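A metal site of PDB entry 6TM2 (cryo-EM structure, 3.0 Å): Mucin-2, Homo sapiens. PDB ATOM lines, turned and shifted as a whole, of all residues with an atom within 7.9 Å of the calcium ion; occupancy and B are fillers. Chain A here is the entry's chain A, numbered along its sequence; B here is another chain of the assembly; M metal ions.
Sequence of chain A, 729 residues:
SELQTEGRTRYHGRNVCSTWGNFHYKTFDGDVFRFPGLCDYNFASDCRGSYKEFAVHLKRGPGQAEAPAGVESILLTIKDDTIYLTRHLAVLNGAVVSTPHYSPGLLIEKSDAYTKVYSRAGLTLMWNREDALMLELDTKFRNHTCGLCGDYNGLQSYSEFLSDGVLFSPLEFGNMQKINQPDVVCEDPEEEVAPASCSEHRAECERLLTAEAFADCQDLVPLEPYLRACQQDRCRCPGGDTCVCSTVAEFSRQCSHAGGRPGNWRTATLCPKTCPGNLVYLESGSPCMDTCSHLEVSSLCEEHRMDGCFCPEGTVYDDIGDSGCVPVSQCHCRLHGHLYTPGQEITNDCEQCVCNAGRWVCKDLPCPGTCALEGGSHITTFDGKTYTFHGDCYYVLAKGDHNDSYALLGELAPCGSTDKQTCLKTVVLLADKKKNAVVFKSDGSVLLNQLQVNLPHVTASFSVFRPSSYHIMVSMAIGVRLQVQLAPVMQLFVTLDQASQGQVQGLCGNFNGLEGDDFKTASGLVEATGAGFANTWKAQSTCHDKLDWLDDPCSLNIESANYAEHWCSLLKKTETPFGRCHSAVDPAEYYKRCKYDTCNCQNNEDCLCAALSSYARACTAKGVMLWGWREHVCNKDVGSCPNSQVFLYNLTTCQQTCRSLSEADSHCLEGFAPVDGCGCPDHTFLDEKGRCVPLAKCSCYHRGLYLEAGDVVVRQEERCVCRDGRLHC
The backbone NH (N) of Gly 502 sits close to the backbone carbonyl oxygen (O) of Asn 510 (3.3 Å).
The backbone NH (N) of Asn 512 sits at hydrogen-bond distance from the side-chain carboxylate (OD2) of Asp 383, 3.0 Å away.
The side-chain carboxylate of Asp 518 is in hydrogen-bond range of the side-chain hydroxyl of Thr 381 (3.1 Å).
The side-chain carboxylate of Asp 383 is in hydrogen-bond range of the backbone NH of Gly 513.
OG1 of Thr 381 lies close to N of Asp 383 (3.4 Å).
Merely in contact with the calcium ion: Asp 383 (3.2 Å).
Six residues have an atom within 4 Å of the calcium ion: Asp 383, Asn 510, Asn 512, Leu 514, Asp 517 and Asp 518.
The nearest printed residue that does not touch the calcium ion is Phe 511 (4.3 Å).
The calcium ion is bound by the backbone carbonyl oxygen (O) of Leu 514 (2.4 Å), the side-chain amide oxygen (OD1) of Asn 510 (2.5 Å), the side-chain amide oxygen (OD1) of Asn 512 (2.5 Å), the side-chain carboxylate (OD1) of Asp 518 (2.5 Å) and the side-chain carboxylate (OD1) of Asp 517 (2.6 Å).
The calcium ion has five donor atoms within binding distance.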
ATOM      1  N   THR A 381       5.951  -5.641   8.421  1.00  0.00           N
ATOM      2  CA  THR A 381       4.996  -6.105   7.429  1.00  0.00           C
ATOM      3  C   THR A 381       3.842  -5.117   7.312  1.00  0.00           C
ATOM      4  O   THR A 381       3.816  -4.085   7.980  1.00  0.00           O
ATOM      5  CB  THR A 381       4.491  -7.502   7.781  1.00  0.00           C
ATOM      6  OG1 THR A 381       3.748  -7.433   8.998  1.00  0.00           O
ATOM      7  CG2 THR A 381       5.634  -8.453   7.991  1.00  0.00           C
ATOM      8  N   PHE A 382       2.862  -5.445   6.471  1.00  0.00           N
ATOM      9  CA  PHE A 382       1.704  -4.577   6.341  1.00  0.00           C
ATOM     10  C   PHE A 382       0.804  -4.592   7.563  1.00  0.00           C
ATOM     11  O   PHE A 382      -0.051  -3.701   7.686  1.00  0.00           O
ATOM     12  CB  PHE A 382       0.858  -4.959   5.138  1.00  0.00           C
ATOM     13  CG  PHE A 382       1.479  -4.696   3.802  1.00  0.00           C
ATOM     14  CD1 PHE A 382       1.523  -3.411   3.296  1.00  0.00           C
ATOM     15  CD2 PHE A 382       1.893  -5.731   2.998  1.00  0.00           C
ATOM     16  CE1 PHE A 382       2.061  -3.165   2.057  1.00  0.00           C
ATOM     17  CE2 PHE A 382       2.426  -5.483   1.750  1.00  0.00           C
ATOM     18  CZ  PHE A 382       2.512  -4.196   1.291  1.00  0.00           C
ATOM     19  N   ASP A 383       0.938  -5.565   8.447  1.00  0.00           N
ATOM     20  CA  ASP A 383       0.041  -5.767   9.583  1.00  0.00           C
ATOM     21  C   ASP A 383       0.777  -5.652  10.905  1.00  0.00           C
ATOM     22  O   ASP A 383       0.488  -6.392  11.844  1.00  0.00           O
ATOM     23  CB  ASP A 383      -0.644  -7.129   9.495  1.00  0.00           C
ATOM     24  CG  ASP A 383      -1.624  -7.209   8.365  1.00  0.00           C
ATOM     25  OD1 ASP A 383      -2.181  -6.160   8.003  1.00  0.00           O
ATOM     26  OD2 ASP A 383      -1.851  -8.312   7.846  1.00  0.00           O
ATOM     27  N   LYS A 385       4.082  -6.373  12.975  1.00  0.00           N
ATOM     28  CA  LYS A 385       4.939  -7.567  12.871  1.00  0.00           C
ATOM     29  C   LYS A 385       6.339  -7.205  12.365  1.00  0.00           C
ATOM     30  O   LYS A 385       6.678  -7.384  11.196  1.00  0.00           O
ATOM     31  CB  LYS A 385       4.235  -8.619  12.004  1.00  0.00           C
ATOM     32  CG  LYS A 385       4.913  -9.987  11.919  1.00  0.00           C
ATOM     33  CD  LYS A 385       4.778 -10.724  13.213  1.00  0.00           C
ATOM     34  CE  LYS A 385       5.286 -12.131  13.087  1.00  0.00           C
ATOM     35  NZ  LYS A 385       5.162 -12.839  14.378  1.00  0.00           N
ATOM     36  N   GLY A 502      -5.384  -8.948   1.495  1.00  0.00           N
ATOM     37  CA  GLY A 502      -5.404 -10.388   1.362  1.00  0.00           C
ATOM     38  C   GLY A 502      -5.023 -10.893  -0.005  1.00  0.00           C
ATOM     39  O   GLY A 502      -5.367 -12.025  -0.348  1.00  0.00           O
ATOM     40  N   CYS A 508       6.581  -9.180   3.022  1.00  0.00           N
ATOM     41  CA  CYS A 508       5.748  -8.180   3.655  1.00  0.00           C
ATOM     42  C   CYS A 508       4.436  -8.754   4.174  1.00  0.00           C
ATOM     43  O   CYS A 508       3.593  -7.985   4.630  1.00  0.00           O
ATOM     44  CB  CYS A 508       5.464  -7.045   2.684  1.00  0.00           C
ATOM     45  SG  CYS A 508       6.864  -5.994   2.288  1.00  0.00           S
ATOM     46  N   GLY A 509       4.247 -10.060   4.115  1.00  0.00           N
ATOM     47  CA  GLY A 509       3.040 -10.666   4.636  1.00  0.00           C
ATOM     48  C   GLY A 509       1.922 -10.657   3.615  1.00  0.00           C
ATOM     49  O   GLY A 509       2.120 -10.397   2.435  1.00  0.00           O
ATOM     50  N   ASN A 510       0.725 -10.959   4.097  1.00  0.00           N
ATOM     51  CA  ASN A 510      -0.429 -11.044   3.217  1.00  0.00           C
ATOM     52  C   ASN A 510      -1.473  -9.956   3.412  1.00  0.00           C
ATOM     53  O   ASN A 510      -2.393  -9.878   2.585  1.00  0.00           O
ATOM     54  CB  ASN A 510      -1.094 -12.429   3.314  1.00  0.00           C
ATOM     55  CG  ASN A 510      -1.520 -12.788   4.707  1.00  0.00           C
ATOM     56  OD1 ASN A 510      -1.384 -12.021   5.643  1.00  0.00           O
ATOM     57  ND2 ASN A 510      -2.049 -13.998   4.848  1.00  0.00           N
ATOM     58  N   PHE A 511      -1.365  -9.133   4.467  1.00  0.00           N
ATOM     59  CA  PHE A 511      -2.193  -7.927   4.672  1.00  0.00           C
ATOM     60  C   PHE A 511      -3.678  -8.295   4.745  1.00  0.00           C
ATOM     61  O   PHE A 511      -4.451  -8.097   3.817  1.00  0.00           O
ATOM     62  CB  PHE A 511      -1.835  -6.894   3.585  1.00  0.00           C
ATOM     63  CG  PHE A 511      -2.624  -5.603   3.634  1.00  0.00           C
ATOM     64  CD1 PHE A 511      -2.611  -4.793   4.747  1.00  0.00           C
ATOM     65  CD2 PHE A 511      -3.190  -5.101   2.475  1.00  0.00           C
ATOM     66  CE1 PHE A 511      -3.277  -3.584   4.757  1.00  0.00           C
ATOM     67  CE2 PHE A 511      -3.840  -3.892   2.474  1.00  0.00           C
ATOM     68  CZ  PHE A 511      -3.883  -3.129   3.616  1.00  0.00           C
ATOM     69  N   ASN A 512      -4.018  -8.959   5.856  1.00  0.00           N
ATOM     70  CA  ASN A 512      -5.387  -9.391   6.120  1.00  0.00           C
ATOM     71  C   ASN A 512      -5.927  -8.990   7.490  1.00  0.00           C
ATOM     72  O   ASN A 512      -7.039  -9.384   7.836  1.00  0.00           O
ATOM     73  CB  ASN A 512      -5.515 -10.908   5.937  1.00  0.00           C
ATOM     74  CG  ASN A 512      -4.593 -11.716   6.850  1.00  0.00           C
ATOM     75  OD1 ASN A 512      -3.842 -11.169   7.659  1.00  0.00           O
ATOM     76  ND2 ASN A 512      -4.674 -13.020   6.736  1.00  0.00           N
ATOM     77  N   GLY A 513      -5.169  -8.232   8.287  1.00  0.00           N
ATOM     78  CA  GLY A 513      -5.608  -7.788   9.587  1.00  0.00           C
ATOM     79  C   GLY A 513      -4.975  -8.519  10.747  1.00  0.00           C
ATOM     80  O   GLY A 513      -4.688  -7.905  11.771  1.00  0.00           O
ATOM     81  N   LEU A 514      -4.760  -9.824  10.615  1.00  0.00           N
ATOM     82  CA  LEU A 514      -4.069 -10.632  11.612  1.00  0.00           C
ATOM     83  C   LEU A 514      -2.572 -10.606  11.335  1.00  0.00           C
ATOM     84  O   LEU A 514      -2.151 -10.614  10.183  1.00  0.00           O
ATOM     85  CB  LEU A 514      -4.591 -12.064  11.566  1.00  0.00           C
ATOM     86  CG  LEU A 514      -4.072 -13.162  12.491  1.00  0.00           C
ATOM     87  CD1 LEU A 514      -4.414 -12.917  13.931  1.00  0.00           C
ATOM     88  CD2 LEU A 514      -4.651 -14.472  12.022  1.00  0.00           C
ATOM     89  N   GLU A 515      -1.764 -10.584  12.386  1.00  0.00           N
ATOM     90  CA  GLU A 515      -0.312 -10.660  12.219  1.00  0.00           C
ATOM     91  C   GLU A 515       0.246 -11.979  12.725  1.00  0.00           C
ATOM     92  O   GLU A 515       1.465 -12.153  12.761  1.00  0.00           O
ATOM     93  CB  GLU A 515       0.392  -9.498  12.922  1.00  0.00           C
ATOM     94  CG  GLU A 515       0.325  -9.538  14.416  1.00  0.00           C
ATOM     95  CD  GLU A 515       1.007  -8.360  15.064  1.00  0.00           C
ATOM     96  OE1 GLU A 515       1.506  -7.494  14.330  1.00  0.00           O
ATOM     97  OE2 GLU A 515       1.061  -8.298  16.306  1.00  0.00           O
ATOM     98  N   GLY A 516      -0.617 -12.907  13.133  1.00  0.00           N
ATOM     99  CA  GLY A 516      -0.140 -14.230  13.510  1.00  0.00           C
ATOM    100  C   GLY A 516       0.193 -15.103  12.316  1.00  0.00           C
ATOM    101  O   GLY A 516       0.993 -16.033  12.448  1.00  0.00           O
ATOM    102  N   ASP A 517      -0.408 -14.819  11.163  1.00  0.00           N
ATOM    103  CA  ASP A 517      -0.180 -15.609   9.961  1.00  0.00           C
ATOM    104  C   ASP A 517       0.694 -14.898   8.939  1.00  0.00           C
ATOM    105  O   ASP A 517       0.587 -15.179   7.750  1.00  0.00           O
ATOM    106  CB  ASP A 517      -1.494 -16.034   9.316  1.00  0.00           C
ATOM    107  CG  ASP A 517      -2.359 -14.858   8.901  1.00  0.00           C
ATOM    108  OD1 ASP A 517      -2.038 -13.692   9.204  1.00  0.00           O
ATOM    109  OD2 ASP A 517      -3.392 -15.111   8.233  1.00  0.00           O
ATOM    110  N   ASP A 518       1.525 -13.944   9.359  1.00  0.00           N
ATOM    111  CA  ASP A 518       2.424 -13.349   8.389  1.00  0.00           C
ATOM    112  C   ASP A 518       3.590 -14.262   8.069  1.00  0.00           C
ATOM    113  O   ASP A 518       4.122 -14.204   6.952  1.00  0.00           O
ATOM    114  CB  ASP A 518       2.930 -11.980   8.851  1.00  0.00           C
ATOM    115  CG  ASP A 518       1.899 -10.881   8.671  1.00  0.00           C
ATOM    116  OD1 ASP A 518       1.063 -10.980   7.770  1.00  0.00           O
ATOM    117  OD2 ASP A 518       1.975  -9.895   9.412  1.00  0.00           O
ATOM    118  N   PHE A 519       3.982 -15.135   8.995  1.00  0.00           N
ATOM    119  CA  PHE A 519       5.027 -16.109   8.731  1.00  0.00           C
ATOM    120  C   PHE A 519       4.499 -17.384   8.094  1.00  0.00           C
ATOM    121  O   PHE A 519       5.138 -18.427   8.192  1.00  0.00           O
ATOM    122  CB  PHE A 519       5.791 -16.457  10.000  1.00  0.00           C
ATOM    123  CG  PHE A 519       6.678 -15.354  10.512  1.00  0.00           C
ATOM    124  CD1 PHE A 519       6.992 -14.272   9.706  1.00  0.00           C
ATOM    125  CD2 PHE A 519       7.232 -15.437  11.755  1.00  0.00           C
ATOM    126  CE1 PHE A 519       7.795 -13.278  10.173  1.00  0.00           C
ATOM    127  CE2 PHE A 519       8.049 -14.444  12.225  1.00  0.00           C
ATOM    128  CZ  PHE A 519       8.332 -13.370  11.426  1.00  0.00           C
ATOM    129  N   LYS A 520       3.335 -17.323   7.464  1.00  0.00           N
ATOM    130  CA  LYS A 520       2.767 -18.447   6.728  1.00  0.00           C
ATOM    131  C   LYS A 520       3.416 -18.548   5.364  1.00  0.00           C
ATOM    132  O   LYS A 520       3.305 -17.631   4.541  1.00  0.00           O
ATOM    133  CB  LYS A 520       1.269 -18.247   6.584  1.00  0.00           C
ATOM    134  CG  LYS A 520       0.546 -19.348   5.900  1.00  0.00           C
ATOM    135  CD  LYS A 520      -0.928 -19.005   5.853  1.00  0.00           C
ATOM    136  CE  LYS A 520      -1.705 -20.056   5.115  1.00  0.00           C
ATOM    137  NZ  LYS A 520      -3.151 -19.685   5.054  1.00  0.00           N
ATOM    138  N   SER B 250      -6.386  -9.557  14.539  1.00  0.00           N
ATOM    139  CA  SER B 250      -5.793  -9.007  15.756  1.00  0.00           C
ATOM    140  C   SER B 250      -5.645  -7.501  15.746  1.00  0.00           C
ATOM    141  O   SER B 250      -5.078  -6.953  16.695  1.00  0.00           O
ATOM    142  CB  SER B 250      -4.428  -9.613  16.015  1.00  0.00           C
ATOM    143  OG  SER B 250      -3.487  -9.126  15.087  1.00  0.00           O
HETATM  144 CA    CA M   1      -1.396 -11.476   8.041  1.00  0.00          CA
